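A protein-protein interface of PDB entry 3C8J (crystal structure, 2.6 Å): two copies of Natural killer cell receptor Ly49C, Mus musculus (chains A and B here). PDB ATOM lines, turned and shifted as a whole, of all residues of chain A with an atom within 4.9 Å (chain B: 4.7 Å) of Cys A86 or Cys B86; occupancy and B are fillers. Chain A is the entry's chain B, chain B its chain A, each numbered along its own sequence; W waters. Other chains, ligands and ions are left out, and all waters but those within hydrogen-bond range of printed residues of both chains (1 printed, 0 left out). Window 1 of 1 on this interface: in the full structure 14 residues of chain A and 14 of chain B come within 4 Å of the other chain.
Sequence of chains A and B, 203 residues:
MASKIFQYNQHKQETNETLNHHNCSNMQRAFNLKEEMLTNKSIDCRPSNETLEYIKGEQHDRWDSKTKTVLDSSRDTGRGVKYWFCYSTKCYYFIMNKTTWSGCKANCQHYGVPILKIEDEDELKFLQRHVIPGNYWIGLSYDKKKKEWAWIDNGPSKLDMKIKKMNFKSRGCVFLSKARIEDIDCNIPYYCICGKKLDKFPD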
ATOM      1  N   TRP A  84      10.618 -28.321   8.496  1.00  0.00           N
ATOM      2  CA  TRP A  84      11.219 -27.530   9.561  1.00  0.00           C
ATOM      3  C   TRP A  84      11.830 -28.370  10.674  1.00  0.00           C
ATOM      4  O   TRP A  84      11.475 -29.551  10.864  1.00  0.00           O
ATOM      5  CB  TRP A  84      10.224 -26.528  10.142  1.00  0.00           C
ATOM      6  CG  TRP A  84       8.956 -27.085  10.682  1.00  0.00           C
ATOM      7  CD1 TRP A  84       7.846 -27.496   9.961  1.00  0.00           C
ATOM      8  CD2 TRP A  84       8.614 -27.256  12.060  1.00  0.00           C
ATOM      9  NE1 TRP A  84       6.851 -27.930  10.819  1.00  0.00           N
ATOM     10  CE2 TRP A  84       7.291 -27.784  12.109  1.00  0.00           C
ATOM     11  CE3 TRP A  84       9.287 -27.012  13.255  1.00  0.00           C
ATOM     12  CZ2 TRP A  84       6.650 -28.066  13.295  1.00  0.00           C
ATOM     13  CZ3 TRP A  84       8.647 -27.295  14.435  1.00  0.00           C
ATOM     14  CH2 TRP A  84       7.340 -27.823  14.448  1.00  0.00           C
ATOM     15  N   PHE A  85      12.722 -27.735  11.427  1.00  0.00           N
ATOM     16  CA  PHE A  85      13.490 -28.417  12.456  1.00  0.00           C
ATOM     17  C   PHE A  85      13.932 -27.393  13.477  1.00  0.00           C
ATOM     18  O   PHE A  85      14.281 -26.271  13.106  1.00  0.00           O
ATOM     19  CB  PHE A  85      14.715 -28.989  11.768  1.00  0.00           C
ATOM     20  CG  PHE A  85      15.392 -30.071  12.507  1.00  0.00           C
ATOM     21  CD1 PHE A  85      15.114 -31.397  12.213  1.00  0.00           C
ATOM     22  CD2 PHE A  85      16.375 -29.780  13.431  1.00  0.00           C
ATOM     23  CE1 PHE A  85      15.772 -32.422  12.872  1.00  0.00           C
ATOM     24  CE2 PHE A  85      17.041 -30.816  14.096  1.00  0.00           C
ATOM     25  CZ  PHE A  85      16.723 -32.128  13.817  1.00  0.00           C
ATOM     26  N   CYS A  86      13.905 -27.739  14.734  1.00  0.00           N
ATOM     27  CA  CYS A  86      14.437 -26.762  15.681  1.00  0.00           C
ATOM     28  C   CYS A  86      15.649 -27.395  16.388  1.00  0.00           C
ATOM     29  O   CYS A  86      15.713 -28.621  16.545  1.00  0.00           O
ATOM     30  CB  CYS A  86      13.376 -26.475  16.772  1.00  0.00           C
ATOM     31  SG  CYS A  86      11.800 -25.875  16.173  1.00  0.00           S
ATOM     32  N   TYR A  87      16.471 -26.523  16.863  1.00  0.00           N
ATOM     33  CA  TYR A  87      17.588 -26.992  17.722  1.00  0.00           C
ATOM     34  C   TYR A  87      17.768 -25.964  18.810  1.00  0.00           C
ATOM     35  O   TYR A  87      17.634 -24.754  18.516  1.00  0.00           O
ATOM     36  CB  TYR A  87      18.855 -27.173  16.893  1.00  0.00           C
ATOM     37  CG  TYR A  87      19.907 -28.003  17.610  1.00  0.00           C
ATOM     38  CD1 TYR A  87      19.826 -29.406  17.512  1.00  0.00           C
ATOM     39  CD2 TYR A  87      20.943 -27.431  18.302  1.00  0.00           C
ATOM     40  CE1 TYR A  87      20.767 -30.162  18.208  1.00  0.00           C
ATOM     41  CE2 TYR A  87      21.882 -28.198  18.954  1.00  0.00           C
ATOM     42  CZ  TYR A  87      21.778 -29.562  18.917  1.00  0.00           C
ATOM     43  OH  TYR A  87      22.725 -30.339  19.549  1.00  0.00           O
ATOM     44  N   SER A  88      18.121 -26.363  20.011  1.00  0.00           N
ATOM     45  CA  SER A  88      18.304 -25.308  21.043  1.00  0.00           C
ATOM     46  C   SER A  88      17.184 -24.335  20.958  1.00  0.00           C
ATOM     47  O   SER A  88      16.012 -24.789  21.123  1.00  0.00           O
ATOM     48  CB  SER A  88      19.715 -24.826  21.001  1.00  0.00           C
ATOM     49  OG  SER A  88      20.061 -24.071  22.156  1.00  0.00           O
ATOM     50  N   LYS A  90      16.177 -22.208  18.546  1.00  0.00           N
ATOM     51  CA  LYS A  90      15.872 -21.606  17.219  1.00  0.00           C
ATOM     52  C   LYS A  90      15.150 -22.635  16.394  1.00  0.00           C
ATOM     53  O   LYS A  90      15.378 -23.844  16.550  1.00  0.00           O
ATOM     54  CB  LYS A  90      17.233 -21.239  16.592  1.00  0.00           C
ATOM     55  CG  LYS A  90      17.124 -20.220  15.487  1.00  0.00           C
ATOM     56  CD  LYS A  90      18.479 -19.811  14.938  1.00  0.00           C
ATOM     57  CE  LYS A  90      18.314 -18.672  13.935  1.00  0.00           C
ATOM     58  NZ  LYS A  90      19.618 -18.168  13.431  1.00  0.00           N
ATOM     59  N   CYS A  91      14.286 -22.222  15.473  1.00  0.00           N
ATOM     60  CA  CYS A  91      13.760 -23.172  14.457  1.00  0.00           C
ATOM     61  C   CYS A  91      14.042 -22.714  13.042  1.00  0.00           C
ATOM     62  O   CYS A  91      14.086 -21.518  12.758  1.00  0.00           O
ATOM     63  CB  CYS A  91      12.264 -23.440  14.578  1.00  0.00           C
ATOM     64  SG  CYS A  91      11.757 -23.974  16.180  1.00  0.00           S
ATOM     65  N   TYR A  92      14.194 -23.678  12.147  1.00  0.00           N
ATOM     66  CA  TYR A  92      14.608 -23.394  10.784  1.00  0.00           C
ATOM     67  C   TYR A  92      13.634 -24.081   9.859  1.00  0.00           C
ATOM     68  O   TYR A  92      13.022 -25.089  10.224  1.00  0.00           O
ATOM     69  CB  TYR A  92      16.002 -23.940  10.508  1.00  0.00           C
ATOM     70  CG  TYR A  92      17.076 -23.562  11.515  1.00  0.00           C
ATOM     71  CD1 TYR A  92      17.206 -24.247  12.720  1.00  0.00           C
ATOM     72  CD2 TYR A  92      17.985 -22.551  11.239  1.00  0.00           C
ATOM     73  CE1 TYR A  92      18.183 -23.916  13.626  1.00  0.00           C
ATOM     74  CE2 TYR A  92      18.957 -22.197  12.142  1.00  0.00           C
ATOM     75  CZ  TYR A  92      19.042 -22.874  13.334  1.00  0.00           C
ATOM     76  OH  TYR A  92      20.013 -22.525  14.228  1.00  0.00           O
ATOM     77  N   LEU A 198      13.632 -18.332  18.707  1.00  0.00           N
ATOM     78  CA  LEU A 198      12.488 -18.398  19.625  1.00  0.00           C
ATOM     79  C   LEU A 198      12.740 -17.455  20.798  1.00  0.00           C
ATOM     80  O   LEU A 198      13.881 -17.323  21.259  1.00  0.00           O
ATOM     81  CB  LEU A 198      12.264 -19.826  20.147  1.00  0.00           C
ATOM     82  CG  LEU A 198      11.988 -20.892  19.077  1.00  0.00           C
ATOM     83  CD1 LEU A 198      11.640 -22.254  19.697  1.00  0.00           C
ATOM     84  CD2 LEU A 198      10.883 -20.430  18.093  1.00  0.00           C
ATOM     85  N   PRO A 202       7.778 -22.612  23.086  1.00  0.00           N
ATOM     86  CA  PRO A 202       6.674 -22.685  22.137  1.00  0.00           C
ATOM     87  C   PRO A 202       5.389 -23.118  22.810  1.00  0.00           C
ATOM     88  O   PRO A 202       5.350 -24.185  23.441  1.00  0.00           O
ATOM     89  CB  PRO A 202       7.131 -23.749  21.167  1.00  0.00           C
ATOM     90  CG  PRO A 202       8.594 -23.727  21.241  1.00  0.00           C
ATOM     91  CD  PRO A 202       8.936 -23.396  22.636  1.00  0.00           C
ATOM     92  N   TRP B  84      15.378 -24.713  28.846  1.00  0.00           N
ATOM     93  CA  TRP B  84      14.681 -25.420  27.804  1.00  0.00           C
ATOM     94  C   TRP B  84      15.455 -25.430  26.482  1.00  0.00           C
ATOM     95  O   TRP B  84      16.324 -24.592  26.258  1.00  0.00           O
ATOM     96  CB  TRP B  84      13.265 -24.880  27.638  1.00  0.00           C
ATOM     97  CG  TRP B  84      13.188 -23.434  27.238  1.00  0.00           C
ATOM     98  CD1 TRP B  84      13.246 -22.338  28.073  1.00  0.00           C
ATOM     99  CD2 TRP B  84      13.035 -22.922  25.922  1.00  0.00           C
ATOM    100  NE1 TRP B  84      13.141 -21.178  27.350  1.00  0.00           N
ATOM    101  CE2 TRP B  84      12.996 -21.501  26.026  1.00  0.00           C
ATOM    102  CE3 TRP B  84      12.908 -23.512  24.662  1.00  0.00           C
ATOM    103  CZ2 TRP B  84      12.827 -20.672  24.914  1.00  0.00           C
ATOM    104  CZ3 TRP B  84      12.745 -22.678  23.546  1.00  0.00           C
ATOM    105  CH2 TRP B  84      12.709 -21.275  23.688  1.00  0.00           C
ATOM    106  N   PHE B  85      15.106 -26.374  25.608  1.00  0.00           N
ATOM    107  CA  PHE B  85      15.901 -26.718  24.434  1.00  0.00           C
ATOM    108  C   PHE B  85      15.014 -27.525  23.475  1.00  0.00           C
ATOM    109  O   PHE B  85      14.301 -28.461  23.887  1.00  0.00           O
ATOM    110  CB  PHE B  85      17.076 -27.594  24.896  1.00  0.00           C
ATOM    111  CG  PHE B  85      18.207 -27.708  23.902  1.00  0.00           C
ATOM    112  CD1 PHE B  85      19.322 -26.848  23.979  1.00  0.00           C
ATOM    113  CD2 PHE B  85      18.199 -28.707  22.913  1.00  0.00           C
ATOM    114  CE1 PHE B  85      20.378 -26.987  23.099  1.00  0.00           C
ATOM    115  CE2 PHE B  85      19.263 -28.805  21.991  1.00  0.00           C
ATOM    116  CZ  PHE B  85      20.333 -27.956  22.096  1.00  0.00           C
ATOM    117  N   CYS B  86      15.039 -27.164  22.202  1.00  0.00           N
ATOM    118  CA  CYS B  86      14.232 -27.870  21.225  1.00  0.00           C
ATOM    119  C   CYS B  86      15.105 -28.750  20.360  1.00  0.00           C
ATOM    120  O   CYS B  86      16.314 -28.565  20.276  1.00  0.00           O
ATOM    121  CB  CYS B  86      13.447 -26.900  20.369  1.00  0.00           C
ATOM    122  SG  CYS B  86      12.436 -25.854  21.356  1.00  0.00           S
ATOM    123  N   TYR B  87      14.478 -29.723  19.726  1.00  0.00           N
ATOM    124  CA  TYR B  87      15.176 -30.616  18.861  1.00  0.00           C
ATOM    125  C   TYR B  87      14.162 -31.222  17.936  1.00  0.00           C
ATOM    126  O   TYR B  87      13.148 -31.764  18.380  1.00  0.00           O
ATOM    127  CB  TYR B  87      15.935 -31.693  19.653  1.00  0.00           C
ATOM    128  CG  TYR B  87      16.745 -32.569  18.738  1.00  0.00           C
ATOM    129  CD1 TYR B  87      17.838 -32.047  18.044  1.00  0.00           C
ATOM    130  CD2 TYR B  87      16.384 -33.910  18.502  1.00  0.00           C
ATOM    131  CE1 TYR B  87      18.564 -32.821  17.153  1.00  0.00           C
ATOM    132  CE2 TYR B  87      17.126 -34.700  17.601  1.00  0.00           C
ATOM    133  CZ  TYR B  87      18.208 -34.128  16.938  1.00  0.00           C
ATOM    134  OH  TYR B  87      18.973 -34.861  16.070  1.00  0.00           O
ATOM    135  N   SER B  88      14.433 -31.103  16.642  1.00  0.00           N
ATOM    136  CA  SER B  88      13.528 -31.594  15.616  1.00  0.00           C
ATOM    137  C   SER B  88      12.218 -30.839  15.784  1.00  0.00           C
ATOM    138  O   SER B  88      12.231 -29.614  15.823  1.00  0.00           O
ATOM    139  CB  SER B  88      13.375 -33.125  15.723  1.00  0.00           C
ATOM    140  OG  SER B  88      12.832 -33.670  14.545  1.00  0.00           O
ATOM    141  N   LYS B  90      10.231 -30.998  18.574  1.00  0.00           N
ATOM    142  CA  LYS B  90       9.834 -31.199  19.975  1.00  0.00           C
ATOM    143  C   LYS B  90      10.628 -30.254  20.891  1.00  0.00           C
ATOM    144  O   LYS B  90      11.779 -29.931  20.593  1.00  0.00           O
ATOM    145  CB  LYS B  90      10.143 -32.645  20.327  1.00  0.00           C
ATOM    146  CG  LYS B  90       9.361 -33.160  21.464  1.00  0.00           C
ATOM    147  CD  LYS B  90       9.528 -34.675  21.696  1.00  0.00           C
ATOM    148  CE  LYS B  90       8.899 -35.042  23.052  1.00  0.00           C
ATOM    149  NZ  LYS B  90       8.776 -36.513  23.263  1.00  0.00           N
ATOM    150  N   CYS B  91      10.055 -29.813  22.010  1.00  0.00           N
ATOM    151  CA  CYS B  91      10.885 -29.086  22.991  1.00  0.00           C
ATOM    152  C   CYS B  91      10.820 -29.698  24.368  1.00  0.00           C
ATOM    153  O   CYS B  91       9.814 -30.324  24.728  1.00  0.00           O
ATOM    154  CB  CYS B  91      10.577 -27.589  23.076  1.00  0.00           C
ATOM    155  SG  CYS B  91      10.606 -26.738  21.504  1.00  0.00           S
ATOM    156  N   LEU B 198       5.652 -30.176  19.161  1.00  0.00           N
ATOM    157  CA  LEU B 198       5.114 -29.003  18.535  1.00  0.00           C
ATOM    158  C   LEU B 198       4.110 -29.434  17.487  1.00  0.00           C
ATOM    159  O   LEU B 198       4.333 -30.404  16.758  1.00  0.00           O
ATOM    160  CB  LEU B 198       6.220 -28.153  17.910  1.00  0.00           C
ATOM    161  CG  LEU B 198       7.368 -27.810  18.863  1.00  0.00           C
ATOM    162  CD1 LEU B 198       8.372 -26.948  18.192  1.00  0.00           C
ATOM    163  CD2 LEU B 198       6.853 -27.149  20.121  1.00  0.00           C
ATOM    164  N   PRO B 202       6.518 -22.791  15.488  1.00  0.00           N
ATOM    165  CA  PRO B 202       6.327 -21.782  16.530  1.00  0.00           C
ATOM    166  C   PRO B 202       6.109 -20.367  15.997  1.00  0.00           C
ATOM    167  O   PRO B 202       6.942 -19.835  15.257  1.00  0.00           O
ATOM    168  CB  PRO B 202       7.615 -21.877  17.337  1.00  0.00           C
ATOM    169  CG  PRO B 202       8.028 -23.339  17.189  1.00  0.00           C
ATOM    170  CD  PRO B 202       7.691 -23.646  15.761  1.00  0.00           C
HETATM  171  O   HOH W   1      12.323 -32.345  11.741  1.00  0.00           O
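N of Cys B86 sits at hydrogen-bond distance from O of Ser A88 (2.8 Å). The backbone carbonyl oxygen (O) of Ser B88 lies within hydrogen-bond range of the backbone NH (N) of Cys A86.
SG of Cys B91 is disulfide-bonded to SG of Cys B86, at 2.0 Å. The backbone carbonyl oxygen (O) of Phe A85 is in hydrogen-bond range of the backbone NH (N) of Tyr A92, at 2.8 Å. SG of Cys A91 forms a disulfide with SG of Cys A86 (1.9 Å).
Tyr B87 touches Phe A85. CB of Cys A86 touches CB of Cys B86, 3.6 Å away. Tyr B87 touches Cys A86 (CA to O, 3.1 Å). Phe B85 touches Tyr A87. Tyr A87 touches Tyr B87. Phe B85 touches Ser A88 (CE1 to OG, 3.1 Å). SG of Cys A91 touches CG of Pro B202 (3.9 Å). CB of Leu A198 touches CH2 of Trp B84 (3.9 Å). Leu A198 touches Pro B202 (CD2 to CB, 3.7 Å). Leu B198 touches Pro A202.
Of chain B, only Cys B86 (3.6 Å), Tyr B87 (3.1 Å) and Ser B88 (2.7 Å) come within 4 Å of Cys A86. Of the printed residues of chain B, Tyr A87 touches Phe B85, Cys B86 and Tyr B87. Lys A90 touches none of the printed residues of chain B. Cys B86 touches just these residues of chain A: Cys A86 (3.6 Å), Tyr A87 (3.3 Å) and Ser A88 (2.8 Å). Of the printed residues of chain A, Ser B88 touches Phe A85 and Cys A86. Of the printed residues of chain A, Cys B91 touches Pro A202. Of the printed residues of chain A, Pro B202 touches Trp A84 (3.998 Å), Cys A91 (3.9 Å) and Leu A198 (3.7 Å).
Of the 10 printed residues of chain A, 8 touch a printed residue of chain B. Printed residues of chain A that touch a printed residue of chain B: Trp A84, Phe A85, Cys A86, Tyr A87, Ser A88, Cys A91, Leu A198 and Pro A202. Along chain B the printed residues that touch a printed residue of chain A span positions 84 to 202. Among the printed residues, 18 pairs touch across the chains. Among the printed residues, no Asp or Glu carboxylate lies within 4 Å of a Lys or Arg side-chain nitrogen of the other chain.
Phe A85 touches Ser B88, and with the chains exchanged Ser A88 touches Phe B85. Cys B86 touches its own counterpart, Cys A86. Cys A86 touches Tyr B87, and with the chains exchanged Tyr A87 touches Cys B86. Cys A91 touches Pro B202, and with the chains exchanged Pro A202 touches Cys B91. Positions printed for both chains: 84, 85, 86, 87, 88, 90, 91, 198 and 202. Of the 18 pairs that touch across the chains among the printed residues, 18 have their exchanged pair printed and touching as well.
Water W1 bridges O of Trp A84 (3.0 Å) and OG of Ser B88 (3.1 Å).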
